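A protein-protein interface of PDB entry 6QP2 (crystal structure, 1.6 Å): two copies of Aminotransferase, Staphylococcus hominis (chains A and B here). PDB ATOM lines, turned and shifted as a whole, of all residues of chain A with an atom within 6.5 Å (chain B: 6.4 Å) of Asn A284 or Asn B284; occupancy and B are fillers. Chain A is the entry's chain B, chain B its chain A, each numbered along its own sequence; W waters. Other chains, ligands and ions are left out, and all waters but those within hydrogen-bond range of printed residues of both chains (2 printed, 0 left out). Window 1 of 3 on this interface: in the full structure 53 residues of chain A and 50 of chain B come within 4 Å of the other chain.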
ATOM      1  N   GLY A  77      33.485  -3.934 -22.611  1.00  0.00           N
ATOM      2  CA  GLY A  77      32.978  -3.364 -21.380  1.00  0.00           C
ATOM      3  C   GLY A  77      33.288  -1.883 -21.250  1.00  0.00           C
ATOM      4  O   GLY A  77      33.650  -1.202 -22.210  1.00  0.00           O
ATOM      5  N   THR A  79      34.833   1.511 -20.721  1.00  0.00           N
ATOM      6  CA  THR A  79      36.100   1.945 -21.317  1.00  0.00           C
ATOM      7  C   THR A  79      36.289   3.447 -21.047  1.00  0.00           C
ATOM      8  O   THR A  79      35.327   4.234 -21.071  1.00  0.00           O
ATOM      9  CB  THR A  79      36.152   1.622 -22.815  1.00  0.00           C
ATOM     10  OG1 THR A  79      35.926   0.218 -23.010  1.00  0.00           O
ATOM     11  CG2 THR A  79      37.464   2.016 -23.460  1.00  0.00           C
ATOM     12  N   HIS A 111      30.933  12.920 -27.626  1.00  0.00           N
ATOM     13  CA  HIS A 111      30.389  11.932 -28.553  1.00  0.00           C
ATOM     14  C   HIS A 111      29.938  12.635 -29.835  1.00  0.00           C
ATOM     15  O   HIS A 111      28.738  12.652 -30.164  1.00  0.00           O
ATOM     16  CB  HIS A 111      29.254  11.127 -27.913  1.00  0.00           C
ATOM     17  CG  HIS A 111      29.700  10.366 -26.715  1.00  0.00           C
ATOM     18  ND1 HIS A 111      28.847  10.080 -25.663  1.00  0.00           N
ATOM     19  CD2 HIS A 111      30.910   9.857 -26.382  1.00  0.00           C
ATOM     20  CE1 HIS A 111      29.509   9.411 -24.739  1.00  0.00           C
ATOM     21  NE2 HIS A 111      30.782   9.259 -25.153  1.00  0.00           N
ATOM     22  N   GLY A 258      29.961   7.777 -37.596  1.00  0.00           N
ATOM     23  CA  GLY A 258      29.110   6.876 -36.821  1.00  0.00           C
ATOM     24  C   GLY A 258      29.760   6.445 -35.504  1.00  0.00           C
ATOM     25  O   GLY A 258      29.072   6.027 -34.571  1.00  0.00           O
ATOM     26  N   LEU A 259      31.084   6.571 -35.385  1.00  0.00           N
ATOM     27  CA  LEU A 259      31.778   6.149 -34.141  1.00  0.00           C
ATOM     28  C   LEU A 259      31.711   7.226 -33.039  1.00  0.00           C
ATOM     29  O   LEU A 259      32.061   6.937 -31.882  1.00  0.00           O
ATOM     30  CB  LEU A 259      33.211   5.729 -34.480  1.00  0.00           C
ATOM     31  CG  LEU A 259      33.309   4.529 -35.411  1.00  0.00           C
ATOM     32  CD1 LEU A 259      34.731   4.001 -35.447  1.00  0.00           C
ATOM     33  CD2 LEU A 259      32.336   3.412 -35.037  1.00  0.00           C
ATOM     34  N   MET A 260      31.308   8.453 -33.403  1.00  0.00           N
ATOM     35  CA  MET A 260      30.937   9.504 -32.450  1.00  0.00           C
ATOM     36  C   MET A 260      31.979   9.655 -31.344  1.00  0.00           C
ATOM     37  O   MET A 260      31.684   9.451 -30.157  1.00  0.00           O
ATOM     38  CB  MET A 260      29.590   9.165 -31.816  1.00  0.00           C
ATOM     39  CG  MET A 260      28.436   9.262 -32.756  1.00  0.00           C
ATOM     40  SD  MET A 260      26.892   8.969 -31.838  1.00  0.00           S
ATOM     41  CE  MET A 260      27.100   7.243 -31.436  1.00  0.00           C
ATOM     42  N   PHE A 261      33.194  10.020 -31.733  1.00  0.00           N
ATOM     43  CA  PHE A 261      34.241  10.268 -30.782  1.00  0.00           C
ATOM     44  C   PHE A 261      35.053  11.481 -31.242  1.00  0.00           C
ATOM     45  O   PHE A 261      35.551  11.485 -32.344  1.00  0.00           O
ATOM     46  CB  PHE A 261      35.110   9.024 -30.614  1.00  0.00           C
ATOM     47  CG  PHE A 261      36.247   9.185 -29.633  1.00  0.00           C
ATOM     48  CD1 PHE A 261      36.002   9.283 -28.278  1.00  0.00           C
ATOM     49  CD2 PHE A 261      37.559   9.235 -30.070  1.00  0.00           C
ATOM     50  CE1 PHE A 261      37.047   9.416 -27.367  1.00  0.00           C
ATOM     51  CE2 PHE A 261      38.605   9.381 -29.175  1.00  0.00           C
ATOM     52  CZ  PHE A 261      38.352   9.475 -27.817  1.00  0.00           C
ATOM     53  N   THR A 282      33.181   7.210 -19.765  1.00  0.00           N
ATOM     54  CA  THR A 282      32.369   6.221 -20.501  1.00  0.00           C
ATOM     55  C   THR A 282      32.639   6.428 -21.991  1.00  0.00           C
ATOM     56  O   THR A 282      31.960   7.226 -22.582  1.00  0.00           O
ATOM     57  CB  THR A 282      30.905   6.353 -20.074  1.00  0.00           C
ATOM     58  OG1 THR A 282      30.115   6.535 -21.239  1.00  0.00           O
ATOM     59  CG2 THR A 282      30.650   7.552 -19.189  1.00  0.00           C
ATOM     60  N   GLU A 283      33.638   5.732 -22.539  1.00  0.00           N
ATOM     61  CA  GLU A 283      33.952   5.870 -23.980  1.00  0.00           C
ATOM     62  C   GLU A 283      33.686   4.539 -24.683  1.00  0.00           C
ATOM     63  O   GLU A 283      33.572   3.544 -24.016  1.00  0.00           O
ATOM     64  CB  GLU A 283      35.386   6.343 -24.206  1.00  0.00           C
ATOM     65  CG  GLU A 283      35.694   7.728 -23.667  1.00  0.00           C
ATOM     66  CD  GLU A 283      34.733   8.824 -24.075  1.00  0.00           C
ATOM     67  OE1 GLU A 283      34.117   8.697 -25.134  1.00  0.00           O
ATOM     68  OE2 GLU A 283      34.576   9.776 -23.314  1.00  0.00           O
ATOM     69  N   ASN A 284      33.570   4.575 -25.998  1.00  0.00           N
ATOM     70  CA  ASN A 284      33.332   3.355 -26.794  1.00  0.00           C
ATOM     71  C   ASN A 284      34.700   2.795 -27.179  1.00  0.00           C
ATOM     72  O   ASN A 284      35.411   3.458 -27.869  1.00  0.00           O
ATOM     73  CB  ASN A 284      32.443   3.680 -27.989  1.00  0.00           C
ATOM     74  CG  ASN A 284      32.092   2.474 -28.817  1.00  0.00           C
ATOM     75  OD1 ASN A 284      32.920   1.619 -29.023  1.00  0.00           O
ATOM     76  ND2 ASN A 284      30.869   2.430 -29.290  1.00  0.00           N
ATOM     77  N   PRO A 285      35.082   1.596 -26.719  1.00  0.00           N
ATOM     78  CA  PRO A 285      36.399   1.034 -27.043  1.00  0.00           C
ATOM     79  C   PRO A 285      36.678   0.967 -28.556  1.00  0.00           C
ATOM     80  O   PRO A 285      37.830   1.144 -28.985  1.00  0.00           O
ATOM     81  CB  PRO A 285      36.372  -0.386 -26.451  1.00  0.00           C
ATOM     82  CG  PRO A 285      34.889  -0.679 -26.262  1.00  0.00           C
ATOM     83  CD  PRO A 285      34.235   0.653 -25.977  1.00  0.00           C
ATOM     84  N   LEU A 286      35.643   0.682 -29.353  1.00  0.00           N
ATOM     85  CA  LEU A 286      35.806   0.578 -30.799  1.00  0.00           C
ATOM     86  C   LEU A 286      36.054   1.959 -31.408  1.00  0.00           C
ATOM     87  O   LEU A 286      36.852   2.075 -32.346  1.00  0.00           O
ATOM     88  CB  LEU A 286      34.586  -0.095 -31.417  1.00  0.00           C
ATOM     89  CG  LEU A 286      34.278  -1.468 -30.850  1.00  0.00           C
ATOM     90  CD1 LEU A 286      33.193  -2.111 -31.649  1.00  0.00           C
ATOM     91  CD2 LEU A 286      35.515  -2.342 -30.789  1.00  0.00           C
ATOM     92  N   SER A 287      35.403   2.996 -30.863  1.00  0.00           N
ATOM     93  CA  SER A 287      35.557   4.362 -31.352  1.00  0.00           C
ATOM     94  C   SER A 287      36.947   4.905 -31.030  1.00  0.00           C
ATOM     95  O   SER A 287      37.569   5.562 -31.843  1.00  0.00           O
ATOM     96  CB  SER A 287      34.525   5.257 -30.778  1.00  0.00           C
ATOM     97  OG  SER A 287      33.224   4.741 -31.052  1.00  0.00           O
ATOM     98  N   VAL A 288      37.441   4.593 -29.837  1.00  0.00           N
ATOM     99  CA  VAL A 288      38.701   5.063 -29.417  1.00  0.00           C
ATOM    100  C   VAL A 288      39.816   4.398 -30.231  1.00  0.00           C
ATOM    101  O   VAL A 288      40.731   5.092 -30.689  1.00  0.00           O
ATOM    102  CB  VAL A 288      38.919   4.826 -27.912  1.00  0.00           C
ATOM    103  CG1 VAL A 288      40.352   5.173 -27.542  1.00  0.00           C
ATOM    104  CG2 VAL A 288      37.927   5.629 -27.063  1.00  0.00           C
ATOM    105  N   VAL A 289      39.780   3.063 -30.392  1.00  0.00           N
ATOM    106  CA  VAL A 289      40.885   2.391 -31.112  1.00  0.00           C
ATOM    107  C   VAL A 289      40.876   2.851 -32.585  1.00  0.00           C
ATOM    108  O   VAL A 289      41.944   3.006 -33.174  1.00  0.00           O
ATOM    109  CB  VAL A 289      40.903   0.858 -31.003  1.00  0.00           C
ATOM    110  CG1 VAL A 289      40.976   0.364 -29.557  1.00  0.00           C
ATOM    111  CG2 VAL A 289      39.783   0.197 -31.757  1.00  0.00           C
ATOM    112  N   THR B  79      24.492   7.228 -38.919  1.00  0.00           N
ATOM    113  CA  THR B  79      23.574   6.103 -38.784  1.00  0.00           C
ATOM    114  C   THR B  79      22.395   6.507 -37.895  1.00  0.00           C
ATOM    115  O   THR B  79      22.560   7.206 -36.913  1.00  0.00           O
ATOM    116  CB  THR B  79      24.329   4.911 -38.177  1.00  0.00           C
ATOM    117  OG1 THR B  79      25.486   4.718 -38.981  1.00  0.00           O
ATOM    118  CG2 THR B  79      23.500   3.641 -38.088  1.00  0.00           C
ATOM    119  N   HIS B 111      22.582   6.904 -25.300  1.00  0.00           N
ATOM    120  CA  HIS B 111      23.947   6.358 -25.322  1.00  0.00           C
ATOM    121  C   HIS B 111      24.271   5.829 -23.927  1.00  0.00           C
ATOM    122  O   HIS B 111      25.071   6.397 -23.193  1.00  0.00           O
ATOM    123  CB  HIS B 111      24.940   7.418 -25.809  1.00  0.00           C
ATOM    124  CG  HIS B 111      24.641   7.877 -27.198  1.00  0.00           C
ATOM    125  ND1 HIS B 111      25.006   9.127 -27.666  1.00  0.00           N
ATOM    126  CD2 HIS B 111      23.970   7.274 -28.202  1.00  0.00           C
ATOM    127  CE1 HIS B 111      24.588   9.268 -28.905  1.00  0.00           C
ATOM    128  NE2 HIS B 111      23.945   8.141 -29.258  1.00  0.00           N
ATOM    129  N   GLY B 258      30.402  -0.862 -23.280  1.00  0.00           N
ATOM    130  CA  GLY B 258      31.236   0.043 -24.078  1.00  0.00           C
ATOM    131  C   GLY B 258      30.534   0.576 -25.323  1.00  0.00           C
ATOM    132  O   GLY B 258      30.947   1.619 -25.874  1.00  0.00           O
ATOM    133  N   LEU B 259      29.494  -0.122 -25.820  1.00  0.00           N
ATOM    134  CA  LEU B 259      28.894   0.261 -27.085  1.00  0.00           C
ATOM    135  C   LEU B 259      27.818   1.334 -26.869  1.00  0.00           C
ATOM    136  O   LEU B 259      27.417   1.963 -27.810  1.00  0.00           O
ATOM    137  CB  LEU B 259      28.332  -0.976 -27.780  1.00  0.00           C
ATOM    138  CG  LEU B 259      29.377  -2.022 -28.151  1.00  0.00           C
ATOM    139  CD1 LEU B 259      28.728  -3.126 -28.976  1.00  0.00           C
ATOM    140  CD2 LEU B 259      30.527  -1.400 -28.914  1.00  0.00           C
ATOM    141  N   MET B 260      27.419   1.551 -25.609  1.00  0.00           N
ATOM    142  CA  MET B 260      26.625   2.699 -25.192  1.00  0.00           C
ATOM    143  C   MET B 260      25.392   2.913 -26.064  1.00  0.00           C
ATOM    144  O   MET B 260      25.232   3.967 -26.708  1.00  0.00           O
ATOM    145  CB  MET B 260      27.481   3.965 -25.261  1.00  0.00           C
ATOM    146  CG  MET B 260      28.547   3.999 -24.208  1.00  0.00           C
ATOM    147  SD  MET B 260      29.363   5.614 -24.310  1.00  0.00           S
ATOM    148  CE  MET B 260      30.429   5.322 -25.709  1.00  0.00           C
ATOM    149  N   PHE B 261      24.500   1.932 -26.069  1.00  0.00           N
ATOM    150  CA  PHE B 261      23.279   1.990 -26.864  1.00  0.00           C
ATOM    151  C   PHE B 261      22.160   1.358 -26.046  1.00  0.00           C
ATOM    152  O   PHE B 261      22.290   0.205 -25.626  1.00  0.00           O
ATOM    153  CB  PHE B 261      23.458   1.281 -28.214  1.00  0.00           C
ATOM    154  CG  PHE B 261      22.251   1.367 -29.096  1.00  0.00           C
ATOM    155  CD1 PHE B 261      21.831   2.585 -29.607  1.00  0.00           C
ATOM    156  CD2 PHE B 261      21.474   0.250 -29.346  1.00  0.00           C
ATOM    157  CE1 PHE B 261      20.695   2.674 -30.382  1.00  0.00           C
ATOM    158  CE2 PHE B 261      20.341   0.344 -30.131  1.00  0.00           C
ATOM    159  CZ  PHE B 261      19.953   1.557 -30.648  1.00  0.00           C
ATOM    160  N   THR B 282      21.978  10.693 -32.852  1.00  0.00           N
ATOM    161  CA  THR B 282      22.507   9.912 -33.975  1.00  0.00           C
ATOM    162  C   THR B 282      23.136   8.652 -33.360  1.00  0.00           C
ATOM    163  O   THR B 282      23.496   8.680 -32.191  1.00  0.00           O
ATOM    164  CB  THR B 282      23.421  10.803 -34.827  1.00  0.00           C
ATOM    165  OG1 THR B 282      23.828  10.063 -35.979  1.00  0.00           O
ATOM    166  CG2 THR B 282      24.630  11.309 -34.067  1.00  0.00           C
ATOM    167  N   GLU B 283      23.241   7.544 -34.109  1.00  0.00           N
ATOM    168  CA  GLU B 283      23.580   6.253 -33.462  1.00  0.00           C
ATOM    169  C   GLU B 283      24.896   5.705 -34.013  1.00  0.00           C
ATOM    170  O   GLU B 283      25.378   6.103 -35.079  1.00  0.00           O
ATOM    171  CB  GLU B 283      22.433   5.259 -33.615  1.00  0.00           C
ATOM    172  CG  GLU B 283      21.099   5.766 -33.098  1.00  0.00           C
ATOM    173  CD  GLU B 283      21.132   6.361 -31.701  1.00  0.00           C
ATOM    174  OE1 GLU B 283      20.235   7.193 -31.396  1.00  0.00           O
ATOM    175  OE2 GLU B 283      22.070   6.019 -30.923  1.00  0.00           O
ATOM    176  N   ASN B 284      25.508   4.804 -33.250  1.00  0.00           N
ATOM    177  CA  ASN B 284      26.732   4.147 -33.683  1.00  0.00           C
ATOM    178  C   ASN B 284      26.329   2.873 -34.416  1.00  0.00           C
ATOM    179  O   ASN B 284      25.665   2.016 -33.838  1.00  0.00           O
ATOM    180  CB  ASN B 284      27.644   3.894 -32.480  1.00  0.00           C
ATOM    181  CG  ASN B 284      28.981   3.288 -32.818  1.00  0.00           C
ATOM    182  OD1 ASN B 284      29.090   2.462 -33.725  1.00  0.00           O
ATOM    183  ND2 ASN B 284      30.016   3.698 -32.100  1.00  0.00           N
ATOM    184  N   PRO B 285      26.729   2.701 -35.698  1.00  0.00           N
ATOM    185  CA  PRO B 285      26.300   1.533 -36.473  1.00  0.00           C
ATOM    186  C   PRO B 285      26.813   0.231 -35.831  1.00  0.00           C
ATOM    187  O   PRO B 285      26.126  -0.798 -35.883  1.00  0.00           O
ATOM    188  CB  PRO B 285      26.886   1.772 -37.875  1.00  0.00           C
ATOM    189  CG  PRO B 285      28.065   2.690 -37.624  1.00  0.00           C
ATOM    190  CD  PRO B 285      27.661   3.562 -36.448  1.00  0.00           C
ATOM    191  N   LEU B 286      27.990   0.268 -35.211  1.00  0.00           N
ATOM    192  CA  LEU B 286      28.525  -1.003 -34.613  1.00  0.00           C
ATOM    193  C   LEU B 286      27.707  -1.351 -33.367  1.00  0.00           C
ATOM    194  O   LEU B 286      27.424  -2.530 -33.119  1.00  0.00           O
ATOM    195  CB  LEU B 286      30.005  -0.864 -34.291  1.00  0.00           C
ATOM    196  CG  LEU B 286      30.873  -0.419 -35.461  1.00  0.00           C
ATOM    197  CD1 LEU B 286      32.325  -0.372 -35.071  1.00  0.00           C
ATOM    198  CD2 LEU B 286      30.651  -1.343 -36.643  1.00  0.00           C
ATOM    199  N   SER B 287      27.298  -0.321 -32.599  1.00  0.00           N
ATOM    200  CA  SER B 287      26.483  -0.504 -31.397  1.00  0.00           C
ATOM    201  C   SER B 287      25.103  -1.053 -31.772  1.00  0.00           C
ATOM    202  O   SER B 287      24.551  -1.883 -31.062  1.00  0.00           O
ATOM    203  CB  SER B 287      26.388   0.769 -30.585  1.00  0.00           C
ATOM    204  OG  SER B 287      27.675   1.319 -30.360  1.00  0.00           O
ATOM    205  N   VAL B 288      24.504  -0.521 -32.843  1.00  0.00           N
ATOM    206  CA  VAL B 288      23.163  -0.913 -33.230  1.00  0.00           C
ATOM    207  C   VAL B 288      23.190  -2.358 -33.727  1.00  0.00           C
ATOM    208  O   VAL B 288      22.331  -3.173 -33.321  1.00  0.00           O
ATOM    209  CB  VAL B 288      22.555   0.027 -34.285  1.00  0.00           C
ATOM    210  CG1 VAL B 288      21.245  -0.532 -34.806  1.00  0.00           C
ATOM    211  CG2 VAL B 288      22.315   1.412 -33.703  1.00  0.00           C
ATOM    212  N   VAL B 289      24.184  -2.697 -34.542  1.00  0.00           N
ATOM    213  CA  VAL B 289      24.194  -4.060 -35.107  1.00  0.00           C
ATOM    214  C   VAL B 289      24.434  -5.045 -33.961  1.00  0.00           C
ATOM    215  O   VAL B 289      23.862  -6.130 -33.964  1.00  0.00           O
ATOM    216  CB  VAL B 289      25.172  -4.319 -36.266  1.00  0.00           C
ATOM    217  CG1 VAL B 289      24.901  -3.400 -37.446  1.00  0.00           C
ATOM    218  CG2 VAL B 289      26.628  -4.304 -35.866  1.00  0.00           C
HETATM  219  O   HOH W   1      29.315   4.992 -29.522  1.00  0.00           O
HETATM  220  O   HOH W   2      27.749   7.712 -27.789  1.00  0.00           O
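Of chain B, only Gly B258 (3.1 Å), Leu B259 (3.7 Å), Met B260 (3.2 Å), Asn B284 (3.2 Å) and Ser B287 (3.5 Å) come within 4 Å of Asn A284.
Asn B284 touches just these residues of chain A: Gly A258 (3.1 Å), Leu A259 (3.6 Å), Met A260 (3.4 Å), Asn A284 (3.2 Å) and Ser A287 (3.5 Å).
Of the printed residues of chain A, Ser B287 touches Asn A284 (3.5 Å).
Printed residues of chain B within 4 Å of Ser A287: Asn B284 (3.5 Å).
Val A288 touches none of the printed residues of chain B.
The nearest residue of chain B that does not touch Asn A284 is Leu B286 (6.1 Å).
His A111 touches Met B260, and with the chains exchanged Met A260 touches His B111.
Met A260 touches Glu B283, and with the chains exchanged Glu A283 touches Met B260.
Met A260 touches Asn B284, and with the chains exchanged Asn A284 touches Met B260.
Asn A284 touches its own counterpart, Asn B284.
The side-chain hydroxyl of Ser B287 sits at hydrogen-bond distance from the backbone carbonyl oxygen of Leu B259, 2.6 Å away.
The backbone NH (N) of Leu A286 lies within hydrogen-bond range of the side-chain amide oxygen (OD1) of Asn A284 (2.9 Å).
The side-chain carboxylate (OE2) of Glu B283 lies within hydrogen-bond range of a ring nitrogen (NE2) of His B111 (3.3 Å).
OD1 of Asn B284 is in hydrogen-bond range of N of Ser B287, at 3.5 Å.
OE1 of Glu A283 lies within hydrogen-bond range of NE2 of His A111 (3.4 Å).
The backbone carbonyl oxygen (O) of Thr A79 is in hydrogen-bond range of the backbone NH (N) of Glu A283 (2.7 Å).
Water W1 lies within hydrogen-bond range of ND2 of Asn B284 (3.0 Å) and ND2 of Asn A284 (3.0 Å).
Water W2 lies within hydrogen-bond range of a ring nitrogen (ND1) of His B111 (3.1 Å) and a ring nitrogen (ND1) of His A111 (3.4 Å).
The side-chain amide nitrogen (ND2) of Asn B284 lies close to the side-chain amide nitrogen (ND2) of Asn A284, at 3.2 Å.
N of Gly B258 sits close to O of Gly A77 (3.4 Å).
The side-chain sulfur (SD) of Met A260 lies close to the backbone carbonyl oxygen (O) of Thr B282, 3.4 Å away.
OG1 of Thr A282 lies within hydrogen-bond range of SD of Met B260, 3.3 Å away.
CD of Pro B285 touches O of Gly A258 (3.4 Å).
Asn B284 touches Leu A259 (OD1 to CD2, 3.6 Å).
SD of Met A260 touches CE1 of His B111, 3.7 Å away.
Met A260 touches Glu B283 (CE to C, 3.7 Å).
Glu A283 touches Gly B258.
Asn A284 touches Gly B258.
ND2 of Asn A284 touches CA of Leu B259, 3.7 Å away.
ND2 of Asn A284 touches OG of Ser B287, at 3.5 Å.
Leu A286 touches Leu B259.
Asn B284 touches Ser A287.
Hydrophobic or aromatic side chains of chain A that line the printed part of chain B: His A111, Leu A259, Met A260, Pro A285 and Leu A286.
Of the 14 printed residues of chain B, 10 touch a printed residue of chain A.
Hydrophobic or aromatic side chains of chain B within 4 Å of the printed part of chain A: His B111, Leu B259, Met B260, Pro B285 and Leu B286.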
